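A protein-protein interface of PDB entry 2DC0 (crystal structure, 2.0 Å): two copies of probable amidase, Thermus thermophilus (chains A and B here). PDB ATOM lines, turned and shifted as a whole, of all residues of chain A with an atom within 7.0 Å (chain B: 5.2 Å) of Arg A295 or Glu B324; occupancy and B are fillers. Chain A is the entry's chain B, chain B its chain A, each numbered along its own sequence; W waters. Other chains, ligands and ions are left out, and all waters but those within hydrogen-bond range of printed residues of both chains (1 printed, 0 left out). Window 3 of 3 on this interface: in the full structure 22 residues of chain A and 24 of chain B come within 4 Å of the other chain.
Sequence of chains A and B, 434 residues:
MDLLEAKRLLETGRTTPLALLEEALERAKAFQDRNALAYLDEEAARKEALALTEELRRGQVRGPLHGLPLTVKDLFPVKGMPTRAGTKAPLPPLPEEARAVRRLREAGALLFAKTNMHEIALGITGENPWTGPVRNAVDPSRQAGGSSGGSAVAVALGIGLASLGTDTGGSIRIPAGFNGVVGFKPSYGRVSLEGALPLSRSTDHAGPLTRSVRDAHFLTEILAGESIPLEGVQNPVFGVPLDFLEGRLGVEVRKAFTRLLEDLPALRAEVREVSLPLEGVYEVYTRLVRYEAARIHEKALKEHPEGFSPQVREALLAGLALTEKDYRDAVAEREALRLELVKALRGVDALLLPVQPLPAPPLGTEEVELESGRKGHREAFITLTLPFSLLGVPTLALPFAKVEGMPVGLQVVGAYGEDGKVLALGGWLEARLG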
ATOM      1  N   LEU A 199      24.914  12.518  31.104  1.00  0.00           N
ATOM      2  CA  LEU A 199      23.790  11.635  30.819  1.00  0.00           C
ATOM      3  C   LEU A 199      24.067  11.302  29.365  1.00  0.00           C
ATOM      4  O   LEU A 199      24.453  10.185  29.029  1.00  0.00           O
ATOM      5  CB  LEU A 199      22.442  12.348  30.956  1.00  0.00           C
ATOM      6  CG  LEU A 199      21.241  11.497  30.505  1.00  0.00           C
ATOM      7  CD1 LEU A 199      21.137  10.233  31.356  1.00  0.00           C
ATOM      8  CD2 LEU A 199      19.964  12.317  30.605  1.00  0.00           C
ATOM      9  N   VAL A 289      20.480   9.153  23.099  1.00  0.00           N
ATOM     10  CA  VAL A 289      20.594   9.434  24.528  1.00  0.00           C
ATOM     11  C   VAL A 289      20.708   8.175  25.386  1.00  0.00           C
ATOM     12  O   VAL A 289      21.587   8.081  26.242  1.00  0.00           O
ATOM     13  CB  VAL A 289      19.391  10.271  25.015  1.00  0.00           C
ATOM     14  CG1 VAL A 289      19.430  10.424  26.528  1.00  0.00           C
ATOM     15  CG2 VAL A 289      19.418  11.634  24.343  1.00  0.00           C
ATOM     16  N   ARG A 290      19.817   7.213  25.167  1.00  0.00           N
ATOM     17  CA  ARG A 290      19.852   5.980  25.943  1.00  0.00           C
ATOM     18  C   ARG A 290      21.145   5.214  25.710  1.00  0.00           C
ATOM     19  O   ARG A 290      21.695   4.611  26.632  1.00  0.00           O
ATOM     20  CB  ARG A 290      18.646   5.098  25.612  1.00  0.00           C
ATOM     21  CG  ARG A 290      17.334   5.622  26.193  1.00  0.00           C
ATOM     22  CD  ARG A 290      16.197   4.622  26.023  1.00  0.00           C
ATOM     23  NE  ARG A 290      14.927   5.135  26.545  1.00  0.00           N
ATOM     24  CZ  ARG A 290      13.746   4.568  26.319  1.00  0.00           C
ATOM     25  NH1 ARG A 290      13.668   3.467  25.580  1.00  0.00           N
ATOM     26  NH2 ARG A 290      12.643   5.101  26.831  1.00  0.00           N
ATOM     27  N   TYR A 291      21.640   5.233  24.478  1.00  0.00           N
ATOM     28  CA  TYR A 291      22.885   4.540  24.191  1.00  0.00           C
ATOM     29  C   TYR A 291      24.006   5.152  25.037  1.00  0.00           C
ATOM     30  O   TYR A 291      24.734   4.437  25.731  1.00  0.00           O
ATOM     31  CB  TYR A 291      23.237   4.654  22.705  1.00  0.00           C
ATOM     32  CG  TYR A 291      24.516   3.932  22.360  1.00  0.00           C
ATOM     33  CD1 TYR A 291      24.506   2.596  21.953  1.00  0.00           C
ATOM     34  CD2 TYR A 291      25.752   4.564  22.513  1.00  0.00           C
ATOM     35  CE1 TYR A 291      25.701   1.911  21.711  1.00  0.00           C
ATOM     36  CE2 TYR A 291      26.939   3.887  22.277  1.00  0.00           C
ATOM     37  CZ  TYR A 291      26.907   2.565  21.879  1.00  0.00           C
ATOM     38  OH  TYR A 291      28.099   1.905  21.672  1.00  0.00           O
ATOM     39  N   GLU A 292      24.139   6.476  24.987  1.00  0.00           N
ATOM     40  CA  GLU A 292      25.184   7.168  25.750  1.00  0.00           C
ATOM     41  C   GLU A 292      25.007   7.032  27.264  1.00  0.00           C
ATOM     42  O   GLU A 292      25.970   6.767  27.991  1.00  0.00           O
ATOM     43  CB  GLU A 292      25.236   8.662  25.372  1.00  0.00           C
ATOM     44  CG  GLU A 292      25.504   8.934  23.881  1.00  0.00           C
ATOM     45  CD  GLU A 292      25.850  10.395  23.572  1.00  0.00           C
ATOM     46  OE1 GLU A 292      25.477  11.293  24.360  1.00  0.00           O
ATOM     47  OE2 GLU A 292      26.478  10.651  22.519  1.00  0.00           O
ATOM     48  N   ALA A 293      23.777   7.208  27.738  1.00  0.00           N
ATOM     49  CA  ALA A 293      23.484   7.116  29.172  1.00  0.00           C
ATOM     50  C   ALA A 293      23.833   5.743  29.745  1.00  0.00           C
ATOM     51  O   ALA A 293      24.402   5.639  30.836  1.00  0.00           O
ATOM     52  CB  ALA A 293      22.005   7.415  29.423  1.00  0.00           C
ATOM     53  N   ALA A 294      23.469   4.693  29.014  1.00  0.00           N
ATOM     54  CA  ALA A 294      23.748   3.329  29.452  1.00  0.00           C
ATOM     55  C   ALA A 294      25.247   3.093  29.591  1.00  0.00           C
ATOM     56  O   ALA A 294      25.692   2.395  30.502  1.00  0.00           O
ATOM     57  CB  ALA A 294      23.157   2.333  28.467  1.00  0.00           C
ATOM     58  N   ARG A 295      26.029   3.677  28.688  1.00  0.00           N
ATOM     59  CA  ARG A 295      27.473   3.499  28.733  1.00  0.00           C
ATOM     60  C   ARG A 295      28.075   4.259  29.910  1.00  0.00           C
ATOM     61  O   ARG A 295      29.075   3.832  30.498  1.00  0.00           O
ATOM     62  CB  ARG A 295      28.110   3.949  27.410  1.00  0.00           C
ATOM     63  CG  ARG A 295      27.609   3.166  26.180  1.00  0.00           C
ATOM     64  CD  ARG A 295      27.705   1.667  26.435  1.00  0.00           C
ATOM     65  NE  ARG A 295      27.246   0.801  25.338  1.00  0.00           N
ATOM     66  CZ  ARG A 295      26.017   0.792  24.823  1.00  0.00           C
ATOM     67  NH1 ARG A 295      25.083   1.619  25.273  1.00  0.00           N
ATOM     68  NH2 ARG A 295      25.702  -0.094  23.889  1.00  0.00           N
ATOM     69  N   ILE A 296      27.462   5.382  30.270  1.00  0.00           N
ATOM     70  CA  ILE A 296      27.959   6.167  31.403  1.00  0.00           C
ATOM     71  C   ILE A 296      27.802   5.398  32.721  1.00  0.00           C
ATOM     72  O   ILE A 296      28.687   5.428  33.581  1.00  0.00           O
ATOM     73  CB  ILE A 296      27.200   7.505  31.554  1.00  0.00           C
ATOM     74  CG1 ILE A 296      27.488   8.421  30.351  1.00  0.00           C
ATOM     75  CG2 ILE A 296      27.594   8.174  32.878  1.00  0.00           C
ATOM     76  CD1 ILE A 296      26.864   9.816  30.401  1.00  0.00           C
ATOM     77  N   HIS A 297      26.670   4.714  32.870  1.00  0.00           N
ATOM     78  CA  HIS A 297      26.373   3.969  34.094  1.00  0.00           C
ATOM     79  C   HIS A 297      26.523   2.457  33.948  1.00  0.00           C
ATOM     80  O   HIS A 297      26.017   1.700  34.781  1.00  0.00           O
ATOM     81  CB  HIS A 297      24.948   4.288  34.542  1.00  0.00           C
ATOM     82  CG  HIS A 297      24.727   5.733  34.864  1.00  0.00           C
ATOM     83  ND1 HIS A 297      25.141   6.303  36.047  1.00  0.00           N
ATOM     84  CD2 HIS A 297      24.170   6.733  34.138  1.00  0.00           C
ATOM     85  CE1 HIS A 297      24.850   7.593  36.038  1.00  0.00           C
ATOM     86  NE2 HIS A 297      24.260   7.878  34.891  1.00  0.00           N
ATOM     87  N   GLU A 298      27.223   2.025  32.903  1.00  0.00           N
ATOM     88  CA  GLU A 298      27.417   0.600  32.633  1.00  0.00           C
ATOM     89  C   GLU A 298      28.022  -0.195  33.794  1.00  0.00           C
ATOM     90  O   GLU A 298      27.543  -1.282  34.123  1.00  0.00           O
ATOM     91  CB  GLU A 298      28.268   0.421  31.364  1.00  0.00           C
ATOM     92  CG  GLU A 298      28.499  -1.029  30.946  1.00  0.00           C
ATOM     93  CD  GLU A 298      29.064  -1.151  29.535  1.00  0.00           C
ATOM     94  OE1 GLU A 298      29.955  -0.355  29.169  1.00  0.00           O
ATOM     95  OE2 GLU A 298      28.628  -2.053  28.789  1.00  0.00           O
ATOM     96  N   LYS A 299      29.063   0.348  34.417  1.00  0.00           N
ATOM     97  CA  LYS A 299      29.716  -0.327  35.533  1.00  0.00           C
ATOM     98  C   LYS A 299      28.752  -0.514  36.706  1.00  0.00           C
ATOM     99  O   LYS A 299      28.611  -1.619  37.237  1.00  0.00           O
ATOM    100  CB  LYS A 299      30.944   0.475  35.977  1.00  0.00           C
ATOM    101  CG  LYS A 299      31.627  -0.039  37.236  1.00  0.00           C
ATOM    102  CD  LYS A 299      32.811   0.850  37.601  1.00  0.00           C
ATOM    103  CE  LYS A 299      33.321   0.572  39.010  1.00  0.00           C
ATOM    104  NZ  LYS A 299      33.771  -0.837  39.200  1.00  0.00           N
ATOM    105  N   LEU A 316      18.115   1.952  31.108  1.00  0.00           N
ATOM    106  CA  LEU A 316      19.544   1.725  30.929  1.00  0.00           C
ATOM    107  C   LEU A 316      19.817   0.407  30.212  1.00  0.00           C
ATOM    108  O   LEU A 316      20.673   0.335  29.320  1.00  0.00           O
ATOM    109  CB  LEU A 316      20.262   1.729  32.282  1.00  0.00           C
ATOM    110  CG  LEU A 316      20.298   3.072  33.013  1.00  0.00           C
ATOM    111  CD1 LEU A 316      21.058   2.928  34.322  1.00  0.00           C
ATOM    112  CD2 LEU A 316      20.964   4.122  32.121  1.00  0.00           C
ATOM    113  N   ALA A 318      17.864  -1.040  28.223  1.00  0.00           N
ATOM    114  CA  ALA A 318      17.415  -0.876  26.846  1.00  0.00           C
ATOM    115  C   ALA A 318      18.512  -0.164  26.059  1.00  0.00           C
ATOM    116  O   ALA A 318      18.706  -0.425  24.870  1.00  0.00           O
ATOM    117  CB  ALA A 318      16.120  -0.073  26.804  1.00  0.00           C
ATOM    118  N   GLY A 319      19.231   0.730  26.732  1.00  0.00           N
ATOM    119  CA  GLY A 319      20.309   1.448  26.080  1.00  0.00           C
ATOM    120  C   GLY A 319      21.454   0.502  25.776  1.00  0.00           C
ATOM    121  O   GLY A 319      22.076   0.584  24.711  1.00  0.00           O
ATOM    122  N   LEU A 320      21.741  -0.394  26.720  1.00  0.00           N
ATOM    123  CA  LEU A 320      22.808  -1.376  26.550  1.00  0.00           C
ATOM    124  C   LEU A 320      22.499  -2.339  25.416  1.00  0.00           C
ATOM    125  O   LEU A 320      23.409  -2.878  24.784  1.00  0.00           O
ATOM    126  CB  LEU A 320      23.018  -2.180  27.834  1.00  0.00           C
ATOM    127  CG  LEU A 320      23.809  -1.528  28.964  1.00  0.00           C
ATOM    128  CD1 LEU A 320      24.127  -2.599  30.011  1.00  0.00           C
ATOM    129  CD2 LEU A 320      25.109  -0.937  28.424  1.00  0.00           C
ATOM    130  N   ALA A 321      21.209  -2.555  25.173  1.00  0.00           N
ATOM    131  CA  ALA A 321      20.758  -3.445  24.111  1.00  0.00           C
ATOM    132  C   ALA A 321      21.018  -2.806  22.748  1.00  0.00           C
ATOM    133  O   ALA A 321      21.079  -3.498  21.732  1.00  0.00           O
ATOM    134  CB  ALA A 321      19.277  -3.741  24.270  1.00  0.00           C
ATOM    135  N   LEU A 322      21.158  -1.483  22.723  1.00  0.00           N
ATOM    136  CA  LEU A 322      21.422  -0.795  21.464  1.00  0.00           C
ATOM    137  C   LEU A 322      22.878  -1.042  21.075  1.00  0.00           C
ATOM    138  O   LEU A 322      23.777  -0.926  21.907  1.00  0.00           O
ATOM    139  CB  LEU A 322      21.152   0.708  21.602  1.00  0.00           C
ATOM    140  CG  LEU A 322      19.707   1.120  21.922  1.00  0.00           C
ATOM    141  CD1 LEU A 322      19.630   2.628  22.143  1.00  0.00           C
ATOM    142  CD2 LEU A 322      18.788   0.703  20.776  1.00  0.00           C
ATOM    143  N   THR A 323      23.100  -1.392  19.813  1.00  0.00           N
ATOM    144  CA  THR A 323      24.443  -1.677  19.307  1.00  0.00           C
ATOM    145  C   THR A 323      25.158  -0.419  18.835  1.00  0.00           C
ATOM    146  O   THR A 323      24.530   0.609  18.608  1.00  0.00           O
ATOM    147  CB  THR A 323      24.395  -2.637  18.114  1.00  0.00           C
ATOM    148  OG1 THR A 323      23.745  -1.986  17.015  1.00  0.00           O
ATOM    149  CG2 THR A 323      23.622  -3.899  18.476  1.00  0.00           C
ATOM    150  N   GLU A 324      26.477  -0.501  18.682  1.00  0.00           N
ATOM    151  CA  GLU A 324      27.235   0.651  18.218  1.00  0.00           C
ATOM    152  C   GLU A 324      26.718   1.067  16.847  1.00  0.00           C
ATOM    153  O   GLU A 324      26.776   2.240  16.485  1.00  0.00           O
ATOM    154  CB  GLU A 324      28.736   0.331  18.182  1.00  0.00           C
ATOM    155  CG  GLU A 324      29.150  -0.843  17.308  1.00  0.00           C
ATOM    156  CD  GLU A 324      29.227  -0.487  15.831  1.00  0.00           C
ATOM    157  OE1 GLU A 324      29.770   0.597  15.504  1.00  0.00           O
ATOM    158  OE2 GLU A 324      28.756  -1.299  14.998  1.00  0.00           O
ATOM    159  N   TYR A 327      23.903   3.301  17.277  1.00  0.00           N
ATOM    160  CA  TYR A 327      24.422   4.606  17.655  1.00  0.00           C
ATOM    161  C   TYR A 327      24.893   5.371  16.411  1.00  0.00           C
ATOM    162  O   TYR A 327      24.521   6.533  16.214  1.00  0.00           O
ATOM    163  CB  TYR A 327      25.564   4.441  18.660  1.00  0.00           C
ATOM    164  CG  TYR A 327      26.088   5.755  19.199  1.00  0.00           C
ATOM    165  CD1 TYR A 327      25.245   6.640  19.878  1.00  0.00           C
ATOM    166  CD2 TYR A 327      27.416   6.124  19.011  1.00  0.00           C
ATOM    167  CE1 TYR A 327      25.716   7.858  20.355  1.00  0.00           C
ATOM    168  CE2 TYR A 327      27.897   7.343  19.479  1.00  0.00           C
ATOM    169  CZ  TYR A 327      27.042   8.200  20.148  1.00  0.00           C
ATOM    170  OH  TYR A 327      27.512   9.400  20.600  1.00  0.00           O
ATOM    171  N   TYR B 291      36.711   5.683  12.542  1.00  0.00           N
ATOM    172  CA  TYR B 291      35.835   4.755  13.248  1.00  0.00           C
ATOM    173  C   TYR B 291      34.685   4.338  12.339  1.00  0.00           C
ATOM    174  O   TYR B 291      34.417   3.144  12.181  1.00  0.00           O
ATOM    175  CB  TYR B 291      35.253   5.390  14.514  1.00  0.00           C
ATOM    176  CG  TYR B 291      34.320   4.460  15.272  1.00  0.00           C
ATOM    177  CD1 TYR B 291      34.818   3.541  16.196  1.00  0.00           C
ATOM    178  CD2 TYR B 291      32.944   4.471  15.034  1.00  0.00           C
ATOM    179  CE1 TYR B 291      33.972   2.651  16.865  1.00  0.00           C
ATOM    180  CE2 TYR B 291      32.086   3.587  15.698  1.00  0.00           C
ATOM    181  CZ  TYR B 291      32.612   2.680  16.610  1.00  0.00           C
ATOM    182  OH  TYR B 291      31.779   1.802  17.259  1.00  0.00           O
ATOM    183  N   LEU B 322      39.924   1.892  17.504  1.00  0.00           N
ATOM    184  CA  LEU B 322      39.140   2.863  18.260  1.00  0.00           C
ATOM    185  C   LEU B 322      37.861   2.141  18.665  1.00  0.00           C
ATOM    186  O   LEU B 322      37.256   1.445  17.851  1.00  0.00           O
ATOM    187  CB  LEU B 322      38.793   4.080  17.387  1.00  0.00           C
ATOM    188  CG  LEU B 322      39.980   4.938  16.930  1.00  0.00           C
ATOM    189  CD1 LEU B 322      39.517   6.003  15.941  1.00  0.00           C
ATOM    190  CD2 LEU B 322      40.624   5.582  18.154  1.00  0.00           C
ATOM    191  N   THR B 323      37.456   2.309  19.917  1.00  0.00           N
ATOM    192  CA  THR B 323      36.251   1.663  20.428  1.00  0.00           C
ATOM    193  C   THR B 323      35.041   2.581  20.325  1.00  0.00           C
ATOM    194  O   THR B 323      35.172   3.741  19.948  1.00  0.00           O
ATOM    195  CB  THR B 323      36.423   1.299  21.899  1.00  0.00           C
ATOM    196  OG1 THR B 323      36.593   2.505  22.655  1.00  0.00           O
ATOM    197  CG2 THR B 323      37.649   0.417  22.081  1.00  0.00           C
ATOM    198  N   GLU B 324      33.868   2.060  20.674  1.00  0.00           N
ATOM    199  CA  GLU B 324      32.658   2.860  20.626  1.00  0.00           C
ATOM    200  C   GLU B 324      32.751   4.013  21.627  1.00  0.00           C
ATOM    201  O   GLU B 324      32.083   5.040  21.468  1.00  0.00           O
ATOM    202  CB  GLU B 324      31.419   1.981  20.873  1.00  0.00           C
ATOM    203  CG  GLU B 324      31.331   1.287  22.231  1.00  0.00           C
ATOM    204  CD  GLU B 324      30.916   2.239  23.333  1.00  0.00           C
ATOM    205  OE1 GLU B 324      29.901   2.950  23.152  1.00  0.00           O
ATOM    206  OE2 GLU B 324      31.597   2.272  24.378  1.00  0.00           O
ATOM    207  N   LYS B 325      33.589   3.853  22.650  1.00  0.00           N
ATOM    208  CA  LYS B 325      33.788   4.918  23.637  1.00  0.00           C
ATOM    209  C   LYS B 325      34.540   6.066  22.960  1.00  0.00           C
ATOM    210  O   LYS B 325      34.199   7.234  23.143  1.00  0.00           O
ATOM    211  CB  LYS B 325      34.596   4.409  24.841  1.00  0.00           C
ATOM    212  CG  LYS B 325      35.028   5.501  25.835  1.00  0.00           C
ATOM    213  CD  LYS B 325      33.830   6.195  26.476  1.00  0.00           C
ATOM    214  CE  LYS B 325      34.245   7.143  27.605  1.00  0.00           C
ATOM    215  NZ  LYS B 325      35.060   8.307  27.138  1.00  0.00           N
ATOM    216  N   ASP B 326      35.562   5.732  22.176  1.00  0.00           N
ATOM    217  CA  ASP B 326      36.330   6.757  21.472  1.00  0.00           C
ATOM    218  C   ASP B 326      35.401   7.500  20.516  1.00  0.00           C
ATOM    219  O   ASP B 326      35.513   8.709  20.340  1.00  0.00           O
ATOM    220  CB  ASP B 326      37.485   6.134  20.675  1.00  0.00           C
ATOM    221  CG  ASP B 326      38.546   5.519  21.565  1.00  0.00           C
ATOM    222  OD1 ASP B 326      39.038   6.217  22.479  1.00  0.00           O
ATOM    223  OD2 ASP B 326      38.899   4.338  21.349  1.00  0.00           O
ATOM    224  N   TYR B 327      34.484   6.762  19.902  1.00  0.00           N
ATOM    225  CA  TYR B 327      33.539   7.344  18.967  1.00  0.00           C
ATOM    226  C   TYR B 327      32.589   8.294  19.697  1.00  0.00           C
ATOM    227  O   TYR B 327      32.336   9.402  19.228  1.00  0.00           O
ATOM    228  CB  TYR B 327      32.768   6.230  18.251  1.00  0.00           C
ATOM    229  CG  TYR B 327      31.781   6.715  17.217  1.00  0.00           C
ATOM    230  CD1 TYR B 327      32.184   7.526  16.155  1.00  0.00           C
ATOM    231  CD2 TYR B 327      30.439   6.352  17.296  1.00  0.00           C
ATOM    232  CE1 TYR B 327      31.266   7.967  15.195  1.00  0.00           C
ATOM    233  CE2 TYR B 327      29.522   6.784  16.348  1.00  0.00           C
ATOM    234  CZ  TYR B 327      29.938   7.588  15.302  1.00  0.00           C
ATOM    235  OH  TYR B 327      29.017   8.011  14.368  1.00  0.00           O
ATOM    236  N   ARG B 328      32.072   7.876  20.850  1.00  0.00           N
ATOM    237  CA  ARG B 328      31.175   8.738  21.619  1.00  0.00           C
ATOM    238  C   ARG B 328      31.874  10.047  21.980  1.00  0.00           C
ATOM    239  O   ARG B 328      31.264  11.118  21.923  1.00  0.00           O
ATOM    240  CB  ARG B 328      30.702   8.033  22.896  1.00  0.00           C
ATOM    241  CG  ARG B 328      29.599   7.006  22.663  1.00  0.00           C
ATOM    242  CD  ARG B 328      29.028   6.492  23.978  1.00  0.00           C
ATOM    243  NE  ARG B 328      29.850   5.440  24.572  1.00  0.00           N
ATOM    244  CZ  ARG B 328      30.549   5.566  25.696  1.00  0.00           C
ATOM    245  NH1 ARG B 328      30.545   6.709  26.371  1.00  0.00           N
ATOM    246  NH2 ARG B 328      31.242   4.538  26.158  1.00  0.00           N
ATOM    247  N   ASP B 329      33.154   9.955  22.349  1.00  0.00           N
ATOM    248  CA  ASP B 329      33.939  11.139  22.705  1.00  0.00           C
ATOM    249  C   ASP B 329      34.117  12.034  21.482  1.00  0.00           C
ATOM    250  O   ASP B 329      33.986  13.263  21.565  1.00  0.00           O
ATOM    251  CB  ASP B 329      35.323  10.743  23.240  1.00  0.00           C
ATOM    252  CG  ASP B 329      35.262  10.103  24.618  1.00  0.00           C
ATOM    253  OD1 ASP B 329      34.242  10.274  25.312  1.00  0.00           O
ATOM    254  OD2 ASP B 329      36.245   9.439  25.010  1.00  0.00           O
HETATM  255  O   HOH W   1      28.944  11.366  23.353  1.00  0.00           O
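OE1 of Glu A324 sits at hydrogen-bond distance from OH of Tyr B291 (2.9 Å).
The side-chain carboxylate (OE1) of Glu B324 lies within hydrogen-bond range of the side-chain hydroxyl (OH) of Tyr A291.
The side-chain carboxylate of Glu B324 is in salt-bridge range of the guanidinium group of Arg B328, 2.9 Å away.
The backbone carbonyl oxygen (O) of Tyr A291 lies within hydrogen-bond range of the guanidinium group (NH1) of Arg A295 (2.9 Å).
The side-chain carboxylate (OE2) of Glu A292 lies within hydrogen-bond range of the side-chain hydroxyl (OH) of Tyr A327.
The guanidinium group (NH1) of Arg A295 lies within hydrogen-bond range of the backbone carbonyl oxygen (O) of Gly A319, at 3.2 Å.
The guanidinium group (NH2) of Arg A295 is in hydrogen-bond range of the backbone carbonyl oxygen (O) of Leu A322, at 2.9 Å.
Among the printed residues, pairs that only touch across the chains: Arg A295 with Arg B328, Tyr A327 with Tyr B327, Tyr A327 with Arg B328, Tyr A291 with Arg B328 and Arg A295 with Glu B324.
Arg A295 touches two residues of chain B.
Leu A320 touches none of the printed residues of chain B.
Printed residues of chain B within 4 Å of Glu A324: Tyr B291 (2.9 Å).
Of the printed residues of chain B, Tyr A327 touches Tyr B327 and Arg B328.
Printed residues of chain A within 4 Å of Tyr B291: Glu A324.
Of chain A, only Tyr A291 (2.6 Å) and Arg A295 (3.8 Å) come within 4 Å of Glu B324.
Of the printed residues of chain A, Tyr B327 touches Tyr A327 (3.5 Å).
Of the printed residues of chain A, Arg B328 touches Tyr A291 (3.7 Å), Arg A295 (3.4 Å) and Tyr A327 (3.6 Å).
The nearest printed residue of chain B that does not touch Arg A295 is Lys B325 (6.2 Å).
The nearest printed residue of chain A that does not touch Tyr B291 is Tyr A291 (5.7 Å).
Printed residues of chain A that touch a printed residue of chain B: Tyr A291, Arg A295, Glu A324 and Tyr A327.
Of the 9 printed residues of chain B, 4 touch a printed residue of chain A.
Hydrophobic or aromatic side chains of chain B within 4 Å of the printed part of chain A: Tyr B291 and Tyr B327.
Among the printed residues, no Asp or Glu carboxylate lies within 4 Å of a Lys or Arg side-chain nitrogen of the other chain.
Tyr A291 touches Glu B324, and with the chains exchanged Glu A324 touches Tyr B291.
Tyr A327 touches its own counterpart, Tyr B327.
Of the 7 pairs that touch across the chains among the printed residues, 3 have their exchanged pair printed and touching as well.
Water W1 lies within hydrogen-bond range of OE2 of Glu A292 (2.7 Å) and O of Arg B328 (2.7 Å).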
